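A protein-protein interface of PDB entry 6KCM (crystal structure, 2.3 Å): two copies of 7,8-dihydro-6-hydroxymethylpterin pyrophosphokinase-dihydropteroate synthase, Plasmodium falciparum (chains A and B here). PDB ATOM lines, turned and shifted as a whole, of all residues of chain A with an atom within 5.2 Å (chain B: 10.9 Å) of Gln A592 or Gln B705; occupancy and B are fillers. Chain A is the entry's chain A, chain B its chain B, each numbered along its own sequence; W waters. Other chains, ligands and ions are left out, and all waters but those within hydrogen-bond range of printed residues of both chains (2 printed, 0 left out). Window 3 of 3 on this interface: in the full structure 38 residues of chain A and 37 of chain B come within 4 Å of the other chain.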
ATOM      1  N   ILE A 588      14.830  13.136 -22.338  1.00  0.00           N
ATOM      2  CA  ILE A 588      13.997  14.226 -22.889  1.00  0.00           C
ATOM      3  C   ILE A 588      12.865  13.705 -23.786  1.00  0.00           C
ATOM      4  O   ILE A 588      11.682  14.087 -23.638  1.00  0.00           O
ATOM      5  CB  ILE A 588      14.859  15.247 -23.669  1.00  0.00           C
ATOM      6  CG1 ILE A 588      15.833  15.973 -22.713  1.00  0.00           C
ATOM      7  CG2 ILE A 588      13.986  16.231 -24.441  1.00  0.00           C
ATOM      8  CD1 ILE A 588      15.159  16.789 -21.607  1.00  0.00           C
ATOM      9  N   LYS A 589      13.199  12.815 -24.701  1.00  0.00           N
ATOM     10  CA  LYS A 589      12.149  12.309 -25.579  1.00  0.00           C
ATOM     11  C   LYS A 589      11.035  11.586 -24.798  1.00  0.00           C
ATOM     12  O   LYS A 589       9.864  11.675 -25.156  1.00  0.00           O
ATOM     13  CB  LYS A 589      12.744  11.380 -26.619  1.00  0.00           C
ATOM     14  CG  LYS A 589      11.845  11.228 -27.832  1.00  0.00           C
ATOM     15  CD  LYS A 589      12.439  10.251 -28.824  1.00  0.00           C
ATOM     16  CE  LYS A 589      11.370   9.734 -29.779  1.00  0.00           C
ATOM     17  NZ  LYS A 589      11.853   8.409 -30.308  1.00  0.00           N
ATOM     18  N   LEU A 590      11.405  10.855 -23.751  1.00  0.00           N
ATOM     19  CA  LEU A 590      10.407  10.215 -22.902  1.00  0.00           C
ATOM     20  C   LEU A 590       9.494  11.268 -22.250  1.00  0.00           C
ATOM     21  O   LEU A 590       8.283  11.070 -22.152  1.00  0.00           O
ATOM     22  CB  LEU A 590      11.079   9.342 -21.827  1.00  0.00           C
ATOM     23  CG  LEU A 590      11.711   8.013 -22.291  1.00  0.00           C
ATOM     24  CD1 LEU A 590      12.535   7.402 -21.154  1.00  0.00           C
ATOM     25  CD2 LEU A 590      10.639   7.041 -22.803  1.00  0.00           C
ATOM     26  N   LEU A 591      10.088  12.362 -21.783  1.00  0.00           N
ATOM     27  CA  LEU A 591       9.315  13.466 -21.209  1.00  0.00           C
ATOM     28  C   LEU A 591       8.396  14.120 -22.226  1.00  0.00           C
ATOM     29  O   LEU A 591       7.233  14.351 -21.937  1.00  0.00           O
ATOM     30  CB  LEU A 591      10.231  14.512 -20.588  1.00  0.00           C
ATOM     31  CG  LEU A 591      10.776  14.128 -19.233  1.00  0.00           C
ATOM     32  CD1 LEU A 591      11.780  15.192 -18.841  1.00  0.00           C
ATOM     33  CD2 LEU A 591       9.634  14.044 -18.216  1.00  0.00           C
ATOM     34  N   GLN A 592       8.905  14.355 -23.430  1.00  0.00           N
ATOM     35  CA  GLN A 592       8.095  14.924 -24.493  1.00  0.00           C
ATOM     36  C   GLN A 592       6.857  14.097 -24.766  1.00  0.00           C
ATOM     37  O   GLN A 592       5.841  14.650 -25.169  1.00  0.00           O
ATOM     38  CB  GLN A 592       8.897  15.070 -25.772  1.00  0.00           C
ATOM     39  CG  GLN A 592      10.003  16.101 -25.669  1.00  0.00           C
ATOM     40  CD  GLN A 592      10.946  16.034 -26.851  1.00  0.00           C
ATOM     41  OE1 GLN A 592      11.074  14.986 -27.463  1.00  0.00           O
ATOM     42  NE2 GLN A 592      11.612  17.152 -27.178  1.00  0.00           N
ATOM     43  N   ASN A 593       6.933  12.792 -24.512  1.00  0.00           N
ATOM     44  CA  ASN A 593       5.860  11.880 -24.895  1.00  0.00           C
ATOM     45  C   ASN A 593       5.205  11.277 -23.693  1.00  0.00           C
ATOM     46  O   ASN A 593       4.656  10.178 -23.740  1.00  0.00           O
ATOM     47  CB  ASN A 593       6.372  10.794 -25.841  1.00  0.00           C
ATOM     48  CG  ASN A 593       6.906  11.377 -27.149  1.00  0.00           C
ATOM     49  OD1 ASN A 593       8.109  11.598 -27.305  1.00  0.00           O
ATOM     50  ND2 ASN A 593       6.007  11.655 -28.075  1.00  0.00           N
ATOM     51  N   ILE A 594       5.250  12.013 -22.602  1.00  0.00           N
ATOM     52  CA  ILE A 594       4.694  11.533 -21.367  1.00  0.00           C
ATOM     53  C   ILE A 594       3.180  11.324 -21.470  1.00  0.00           C
ATOM     54  O   ILE A 594       2.599  10.597 -20.680  1.00  0.00           O
ATOM     55  CB  ILE A 594       5.114  12.500 -20.217  1.00  0.00           C
ATOM     56  CG1 ILE A 594       5.231  11.759 -18.887  1.00  0.00           C
ATOM     57  CG2 ILE A 594       4.182  13.702 -20.115  1.00  0.00           C
ATOM     58  CD1 ILE A 594       6.336  10.714 -18.875  1.00  0.00           C
ATOM     59  N   HIS A 595       2.542  11.949 -22.462  1.00  0.00           N
ATOM     60  CA  HIS A 595       1.090  11.788 -22.680  1.00  0.00           C
ATOM     61  C   HIS A 595       0.688  10.353 -22.883  1.00  0.00           C
ATOM     62  O   HIS A 595      -0.490  10.007 -22.649  1.00  0.00           O
ATOM     63  CB  HIS A 595       0.585  12.641 -23.866  1.00  0.00           C
ATOM     64  CG  HIS A 595       1.149  12.180 -25.197  1.00  0.00           C
ATOM     65  ND1 HIS A 595       2.353  12.613 -25.668  1.00  0.00           N
ATOM     66  CD2 HIS A 595       0.687  11.232 -26.107  1.00  0.00           C
ATOM     67  CE1 HIS A 595       2.624  11.998 -26.843  1.00  0.00           C
ATOM     68  NE2 HIS A 595       1.600  11.158 -27.118  1.00  0.00           N
ATOM     69  N   TYR A 676       6.347  21.384 -15.977  1.00  0.00           N
ATOM     70  CA  TYR A 676       5.904  20.535 -17.069  1.00  0.00           C
ATOM     71  C   TYR A 676       5.003  19.421 -16.541  1.00  0.00           C
ATOM     72  O   TYR A 676       3.935  19.187 -17.077  1.00  0.00           O
ATOM     73  CB  TYR A 676       7.112  19.963 -17.801  1.00  0.00           C
ATOM     74  CG  TYR A 676       6.785  19.095 -18.998  1.00  0.00           C
ATOM     75  CD1 TYR A 676       6.309  19.655 -20.193  1.00  0.00           C
ATOM     76  CD2 TYR A 676       7.008  17.725 -18.958  1.00  0.00           C
ATOM     77  CE1 TYR A 676       6.021  18.873 -21.295  1.00  0.00           C
ATOM     78  CE2 TYR A 676       6.759  16.935 -20.066  1.00  0.00           C
ATOM     79  CZ  TYR A 676       6.266  17.504 -21.219  1.00  0.00           C
ATOM     80  OH  TYR A 676       6.034  16.708 -22.310  1.00  0.00           O
ATOM     81  N   LYS A 680       1.218  18.329 -17.313  1.00  0.00           N
ATOM     82  CA  LYS A 680       0.973  17.032 -17.938  1.00  0.00           C
ATOM     83  C   LYS A 680       0.165  16.166 -17.000  1.00  0.00           C
ATOM     84  O   LYS A 680      -0.250  15.072 -17.359  1.00  0.00           O
ATOM     85  CB  LYS A 680       2.284  16.370 -18.367  1.00  0.00           C
ATOM     86  CG  LYS A 680       2.932  17.096 -19.546  1.00  0.00           C
ATOM     87  CD  LYS A 680       2.068  16.900 -20.784  1.00  0.00           C
ATOM     88  CE  LYS A 680       2.384  17.868 -21.926  1.00  0.00           C
ATOM     89  NZ  LYS A 680       2.106  17.153 -23.228  1.00  0.00           N
ATOM     90  N   GLU B 387       7.932  34.344 -30.245  1.00  0.00           N
ATOM     91  CA  GLU B 387       8.844  33.200 -30.457  1.00  0.00           C
ATOM     92  C   GLU B 387       9.856  32.878 -29.383  1.00  0.00           C
ATOM     93  O   GLU B 387      10.451  31.807 -29.407  1.00  0.00           O
ATOM     94  CB  GLU B 387       9.529  33.273 -31.811  1.00  0.00           C
ATOM     95  CG  GLU B 387       8.548  32.899 -32.913  1.00  0.00           C
ATOM     96  CD  GLU B 387       9.203  32.718 -34.266  1.00  0.00           C
ATOM     97  OE1 GLU B 387      10.446  32.541 -34.328  1.00  0.00           O
ATOM     98  OE2 GLU B 387       8.462  32.765 -35.265  1.00  0.00           O
ATOM     99  N   TYR B 678       6.670  31.233 -20.153  1.00  0.00           N
ATOM    100  CA  TYR B 678       7.185  30.473 -21.285  1.00  0.00           C
ATOM    101  C   TYR B 678       6.032  29.882 -22.100  1.00  0.00           C
ATOM    102  O   TYR B 678       5.968  30.058 -23.322  1.00  0.00           O
ATOM    103  CB  TYR B 678       8.139  29.342 -20.842  1.00  0.00           C
ATOM    104  CG  TYR B 678       8.581  28.513 -22.026  1.00  0.00           C
ATOM    105  CD1 TYR B 678       9.688  28.893 -22.792  1.00  0.00           C
ATOM    106  CD2 TYR B 678       7.860  27.403 -22.416  1.00  0.00           C
ATOM    107  CE1 TYR B 678      10.083  28.154 -23.909  1.00  0.00           C
ATOM    108  CE2 TYR B 678       8.243  26.649 -23.506  1.00  0.00           C
ATOM    109  CZ  TYR B 678       9.347  27.025 -24.243  1.00  0.00           C
ATOM    110  OH  TYR B 678       9.690  26.290 -25.336  1.00  0.00           O
ATOM    111  N   TYR B 679       5.124  29.172 -21.448  1.00  0.00           N
ATOM    112  CA  TYR B 679       4.020  28.555 -22.208  1.00  0.00           C
ATOM    113  C   TYR B 679       3.048  29.549 -22.774  1.00  0.00           C
ATOM    114  O   TYR B 679       2.403  29.257 -23.782  1.00  0.00           O
ATOM    115  CB  TYR B 679       3.259  27.513 -21.389  1.00  0.00           C
ATOM    116  CG  TYR B 679       4.105  26.312 -21.154  1.00  0.00           C
ATOM    117  CD1 TYR B 679       4.570  25.571 -22.232  1.00  0.00           C
ATOM    118  CD2 TYR B 679       4.477  25.925 -19.863  1.00  0.00           C
ATOM    119  CE1 TYR B 679       5.375  24.474 -22.048  1.00  0.00           C
ATOM    120  CE2 TYR B 679       5.271  24.809 -19.667  1.00  0.00           C
ATOM    121  CZ  TYR B 679       5.714  24.096 -20.771  1.00  0.00           C
ATOM    122  OH  TYR B 679       6.536  22.989 -20.641  1.00  0.00           O
ATOM    123  N   LEU B 697      14.195  28.143 -18.398  1.00  0.00           N
ATOM    124  CA  LEU B 697      13.830  28.353 -19.796  1.00  0.00           C
ATOM    125  C   LEU B 697      14.570  27.385 -20.725  1.00  0.00           C
ATOM    126  O   LEU B 697      14.028  26.959 -21.759  1.00  0.00           O
ATOM    127  CB  LEU B 697      14.008  29.822 -20.229  1.00  0.00           C
ATOM    128  CG  LEU B 697      13.224  30.956 -19.503  1.00  0.00           C
ATOM    129  CD1 LEU B 697      13.501  32.307 -20.139  1.00  0.00           C
ATOM    130  CD2 LEU B 697      11.720  30.748 -19.505  1.00  0.00           C
ATOM    131  N   ASP B 698      15.812  27.053 -20.385  1.00  0.00           N
ATOM    132  CA  ASP B 698      16.585  26.123 -21.211  1.00  0.00           C
ATOM    133  C   ASP B 698      15.957  24.727 -21.200  1.00  0.00           C
ATOM    134  O   ASP B 698      15.822  24.113 -22.231  1.00  0.00           O
ATOM    135  CB  ASP B 698      18.042  26.048 -20.746  1.00  0.00           C
ATOM    136  CG  ASP B 698      18.878  27.271 -21.180  1.00  0.00           C
ATOM    137  OD1 ASP B 698      18.449  28.084 -22.055  1.00  0.00           O
ATOM    138  OD2 ASP B 698      19.988  27.421 -20.631  1.00  0.00           O
ATOM    139  N   VAL B 699      15.542  24.249 -20.031  1.00  0.00           N
ATOM    140  CA  VAL B 699      14.904  22.953 -19.950  1.00  0.00           C
ATOM    141  C   VAL B 699      13.559  22.940 -20.686  1.00  0.00           C
ATOM    142  O   VAL B 699      13.287  22.018 -21.464  1.00  0.00           O
ATOM    143  CB  VAL B 699      14.735  22.507 -18.483  1.00  0.00           C
ATOM    144  CG1 VAL B 699      13.884  21.235 -18.394  1.00  0.00           C
ATOM    145  CG2 VAL B 699      16.097  22.341 -17.788  1.00  0.00           C
ATOM    146  N   LEU B 700      12.712  23.948 -20.470  1.00  0.00           N
ATOM    147  CA  LEU B 700      11.412  23.968 -21.164  1.00  0.00           C
ATOM    148  C   LEU B 700      11.578  24.035 -22.677  1.00  0.00           C
ATOM    149  O   LEU B 700      10.854  23.369 -23.414  1.00  0.00           O
ATOM    150  CB  LEU B 700      10.502  25.085 -20.662  1.00  0.00           C
ATOM    151  CG  LEU B 700      10.160  25.058 -19.156  1.00  0.00           C
ATOM    152  CD1 LEU B 700       9.387  26.303 -18.792  1.00  0.00           C
ATOM    153  CD2 LEU B 700       9.321  23.844 -18.765  1.00  0.00           C
ATOM    154  N   THR B 701      12.549  24.822 -23.136  1.00  0.00           N
ATOM    155  CA  THR B 701      12.844  24.954 -24.559  1.00  0.00           C
ATOM    156  C   THR B 701      13.301  23.603 -25.134  1.00  0.00           C
ATOM    157  O   THR B 701      12.853  23.193 -26.201  1.00  0.00           O
ATOM    158  CB  THR B 701      13.913  26.057 -24.792  1.00  0.00           C
ATOM    159  OG1 THR B 701      13.391  27.326 -24.339  1.00  0.00           O
ATOM    160  CG2 THR B 701      14.279  26.170 -26.277  1.00  0.00           C
ATOM    161  N   LYS B 702      14.183  22.907 -24.417  1.00  0.00           N
ATOM    162  CA  LYS B 702      14.613  21.576 -24.842  1.00  0.00           C
ATOM    163  C   LYS B 702      13.436  20.586 -24.902  1.00  0.00           C
ATOM    164  O   LYS B 702      13.325  19.844 -25.857  1.00  0.00           O
ATOM    165  CB  LYS B 702      15.720  21.052 -23.936  1.00  0.00           C
ATOM    166  CG  LYS B 702      17.082  21.031 -24.595  1.00  0.00           C
ATOM    167  CD  LYS B 702      17.323  19.736 -25.368  1.00  0.00           C
ATOM    168  CE  LYS B 702      18.743  19.724 -25.950  1.00  0.00           C
ATOM    169  NZ  LYS B 702      19.083  18.520 -26.768  1.00  0.00           N
ATOM    170  N   ILE B 703      12.541  20.596 -23.911  1.00  0.00           N
ATOM    171  CA  ILE B 703      11.405  19.695 -23.966  1.00  0.00           C
ATOM    172  C   ILE B 703      10.498  20.016 -25.161  1.00  0.00           C
ATOM    173  O   ILE B 703       9.918  19.097 -25.764  1.00  0.00           O
ATOM    174  CB  ILE B 703      10.608  19.660 -22.657  1.00  0.00           C
ATOM    175  CG1 ILE B 703      11.440  19.015 -21.549  1.00  0.00           C
ATOM    176  CG2 ILE B 703       9.290  18.908 -22.852  1.00  0.00           C
ATOM    177  CD1 ILE B 703      10.898  19.256 -20.162  1.00  0.00           C
ATOM    178  N   ASP B 704      10.389  21.299 -25.521  1.00  0.00           N
ATOM    179  CA  ASP B 704       9.640  21.703 -26.727  1.00  0.00           C
ATOM    180  C   ASP B 704      10.312  21.379 -28.063  1.00  0.00           C
ATOM    181  O   ASP B 704       9.639  21.288 -29.070  1.00  0.00           O
ATOM    182  CB  ASP B 704       9.316  23.203 -26.702  1.00  0.00           C
ATOM    183  CG  ASP B 704       7.980  23.501 -26.067  1.00  0.00           C
ATOM    184  OD1 ASP B 704       7.271  22.557 -25.617  1.00  0.00           O
ATOM    185  OD2 ASP B 704       7.631  24.700 -26.014  1.00  0.00           O
ATOM    186  N   GLN B 705      11.629  21.237 -28.087  1.00  0.00           N
ATOM    187  CA  GLN B 705      12.367  21.031 -29.346  1.00  0.00           C
ATOM    188  C   GLN B 705      12.078  19.632 -29.921  1.00  0.00           C
ATOM    189  O   GLN B 705      12.848  18.690 -29.766  1.00  0.00           O
ATOM    190  CB  GLN B 705      13.857  21.286 -29.109  1.00  0.00           C
ATOM    191  CG  GLN B 705      14.818  20.911 -30.231  1.00  0.00           C
ATOM    192  CD  GLN B 705      16.213  20.595 -29.692  1.00  0.00           C
ATOM    193  OE1 GLN B 705      16.850  21.435 -29.053  1.00  0.00           O
ATOM    194  NE2 GLN B 705      16.684  19.372 -29.935  1.00  0.00           N
ATOM    195  N   VAL B 706      10.916  19.500 -30.544  1.00  0.00           N
ATOM    196  CA  VAL B 706      10.490  18.232 -31.127  1.00  0.00           C
ATOM    197  C   VAL B 706      11.143  18.043 -32.492  1.00  0.00           C
ATOM    198  O   VAL B 706      10.897  18.811 -33.423  1.00  0.00           O
ATOM    199  CB  VAL B 706       8.948  18.132 -31.228  1.00  0.00           C
ATOM    200  CG1 VAL B 706       8.362  17.681 -29.892  1.00  0.00           C
ATOM    201  CG2 VAL B 706       8.327  19.458 -31.698  1.00  0.00           C
ATOM    202  N   LYS B 707      12.004  17.037 -32.586  1.00  0.00           N
ATOM    203  CA  LYS B 707      12.670  16.710 -33.847  1.00  0.00           C
ATOM    204  C   LYS B 707      11.661  16.371 -34.963  1.00  0.00           C
ATOM    205  O   LYS B 707      11.591  17.086 -35.972  1.00  0.00           O
ATOM    206  CB  LYS B 707      13.717  15.608 -33.629  1.00  0.00           C
ATOM    207  CG  LYS B 707      14.814  16.081 -32.687  1.00  0.00           C
ATOM    208  CD  LYS B 707      15.893  15.047 -32.430  1.00  0.00           C
ATOM    209  CE  LYS B 707      16.835  15.554 -31.346  1.00  0.00           C
ATOM    210  NZ  LYS B 707      17.713  14.471 -30.834  1.00  0.00           N
ATOM    211  N   ASP B 708      10.858  15.321 -34.756  1.00  0.00           N
ATOM    212  CA  ASP B 708       9.808  14.941 -35.707  1.00  0.00           C
ATOM    213  C   ASP B 708       8.391  15.215 -35.166  1.00  0.00           C
ATOM    214  O   ASP B 708       7.931  14.516 -34.262  1.00  0.00           O
ATOM    215  CB  ASP B 708       9.969  13.468 -36.126  1.00  0.00           C
ATOM    216  CG  ASP B 708       9.027  13.066 -37.269  1.00  0.00           C
ATOM    217  OD1 ASP B 708       8.347  13.960 -37.840  1.00  0.00           O
ATOM    218  OD2 ASP B 708       8.973  11.850 -37.591  1.00  0.00           O
ATOM    219  N   PRO B 709       7.696  16.233 -35.727  1.00  0.00           N
ATOM    220  CA  PRO B 709       6.330  16.588 -35.293  1.00  0.00           C
ATOM    221  C   PRO B 709       5.279  15.509 -35.546  1.00  0.00           C
ATOM    222  O   PRO B 709       4.173  15.580 -35.000  1.00  0.00           O
ATOM    223  CB  PRO B 709       5.995  17.844 -36.124  1.00  0.00           C
ATOM    224  CG  PRO B 709       6.978  17.860 -37.245  1.00  0.00           C
ATOM    225  CD  PRO B 709       8.221  17.187 -36.726  1.00  0.00           C
ATOM    226  N   ASN B 710       5.610  14.530 -36.380  1.00  0.00           N
ATOM    227  CA  ASN B 710       4.679  13.441 -36.664  1.00  0.00           C
ATOM    228  C   ASN B 710       5.009  12.176 -35.883  1.00  0.00           C
ATOM    229  O   ASN B 710       4.172  11.271 -35.778  1.00  0.00           O
ATOM    230  CB  ASN B 710       4.616  13.159 -38.170  1.00  0.00           C
ATOM    231  CG  ASN B 710       3.962  14.289 -38.940  1.00  0.00           C
ATOM    232  OD1 ASN B 710       2.735  14.465 -38.901  1.00  0.00           O
ATOM    233  ND2 ASN B 710       4.782  15.075 -39.637  1.00  0.00           N
ATOM    234  N   SER B 711       6.218  12.138 -35.314  1.00  0.00           N
ATOM    235  CA  SER B 711       6.728  10.936 -34.662  1.00  0.00           C
ATOM    236  C   SER B 711       5.751  10.324 -33.668  1.00  0.00           C
ATOM    237  O   SER B 711       5.653   9.108 -33.579  1.00  0.00           O
ATOM    238  CB  SER B 711       8.102  11.174 -34.009  1.00  0.00           C
ATOM    239  OG  SER B 711       7.985  11.784 -32.733  1.00  0.00           O
ATOM    240  N   SER B 712       5.016  11.142 -32.929  1.00  0.00           N
ATOM    241  CA  SER B 712       4.222  10.586 -31.838  1.00  0.00           C
ATOM    242  C   SER B 712       3.047   9.727 -32.308  1.00  0.00           C
ATOM    243  O   SER B 712       2.719   8.743 -31.659  1.00  0.00           O
ATOM    244  CB  SER B 712       3.773  11.652 -30.836  1.00  0.00           C
ATOM    245  OG  SER B 712       2.748  12.447 -31.389  1.00  0.00           O
ATOM    246  N   SER B 713       2.425  10.064 -33.431  1.00  0.00           N
ATOM    247  CA  SER B 713       1.346   9.207 -33.934  1.00  0.00           C
ATOM    248  C   SER B 713       1.884   8.092 -34.833  1.00  0.00           C
ATOM    249  O   SER B 713       1.342   6.977 -34.853  1.00  0.00           O
ATOM    250  CB  SER B 713       0.238  10.028 -34.619  1.00  0.00           C
ATOM    251  OG  SER B 713       0.771  10.843 -35.641  1.00  0.00           O
ATOM    252  N   ASP B 715       4.927   6.627 -34.369  1.00  0.00           N
ATOM    253  CA  ASP B 715       5.475   5.631 -33.432  1.00  0.00           C
ATOM    254  C   ASP B 715       4.353   4.865 -32.752  1.00  0.00           C
ATOM    255  O   ASP B 715       4.471   3.668 -32.513  1.00  0.00           O
ATOM    256  CB  ASP B 715       6.383   6.293 -32.399  1.00  0.00           C
ATOM    257  CG  ASP B 715       7.622   6.900 -33.025  1.00  0.00           C
ATOM    258  OD1 ASP B 715       7.914   6.550 -34.197  1.00  0.00           O
ATOM    259  OD2 ASP B 715       8.298   7.739 -32.363  1.00  0.00           O
HETATM  260  O   HOH W   1       2.753   8.694 -29.157  1.00  0.00           O
HETATM  261  O   HOH W   2       9.737   6.144 -29.641  1.00  0.00           O
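Ile A588 touches just one residue of chain B: Lys B702 (3.9 Å).
Of the printed residues of chain B, Gln A592 touches Lys B702 (3.5 Å), Ile B703 (2.9 Å) and Gln B705 (3.3 Å).
Of the printed residues of chain B, Tyr A676 touches Tyr B679 and Ile B703.
Of the printed residues of chain A, Lys B702 touches Ile A588 (3.9 Å) and Gln A592 (3.5 Å).
Of chain A, only Gln A592 (3.3 Å) comes within 4 Å of Gln B705.
Of the printed residues of chain A, Ser B712 touches Asn A593 (3.6 Å).
The nearest printed residue of chain A that does not touch Lys B702 is Lys A589 (7.1 Å).
The backbone carbonyl oxygen (O) of Lys A589 lies close to the side-chain amide oxygen (OD1) of Asn A593 (2.8 Å).
O of Leu A591 is in hydrogen-bond range of OH of Tyr A676, at 2.7 Å.
Among the printed residues, merely in contact across the chains: Ile A588 with Lys B702, Asn A593 with Ser B712, Tyr A676 with Tyr B679 and Tyr A676 with Ile B703.
Water W1 lies within hydrogen-bond range of O of Ser B712 and NE2 of His A595.
Water W2 bridges NZ of Lys A589 and OD2 of Asp B715.
The backbone carbonyl oxygen (O) of Gln B705 sits at hydrogen-bond distance from the side-chain amide nitrogen (NE2) of Gln A592, at 3.3 Å.
The side-chain amide nitrogen (NE2) of Gln A592 sits at hydrogen-bond distance from the backbone carbonyl oxygen (O) of Lys B702 (3.5 Å).
The backbone carbonyl oxygen of Ile B703 lies within hydrogen-bond range of the side-chain amide nitrogen of Gln A592 (2.9 Å).
Hydrophobic or aromatic side chains of chain B that line the printed part of chain A: Tyr B679 and Ile B703.
Among the printed residues, 7 pairs touch across the chains.
No position is printed for both chains.
Of the 7 pairs that touch across the chains among the printed residues, none has its exchanged pair printed and touching as well.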
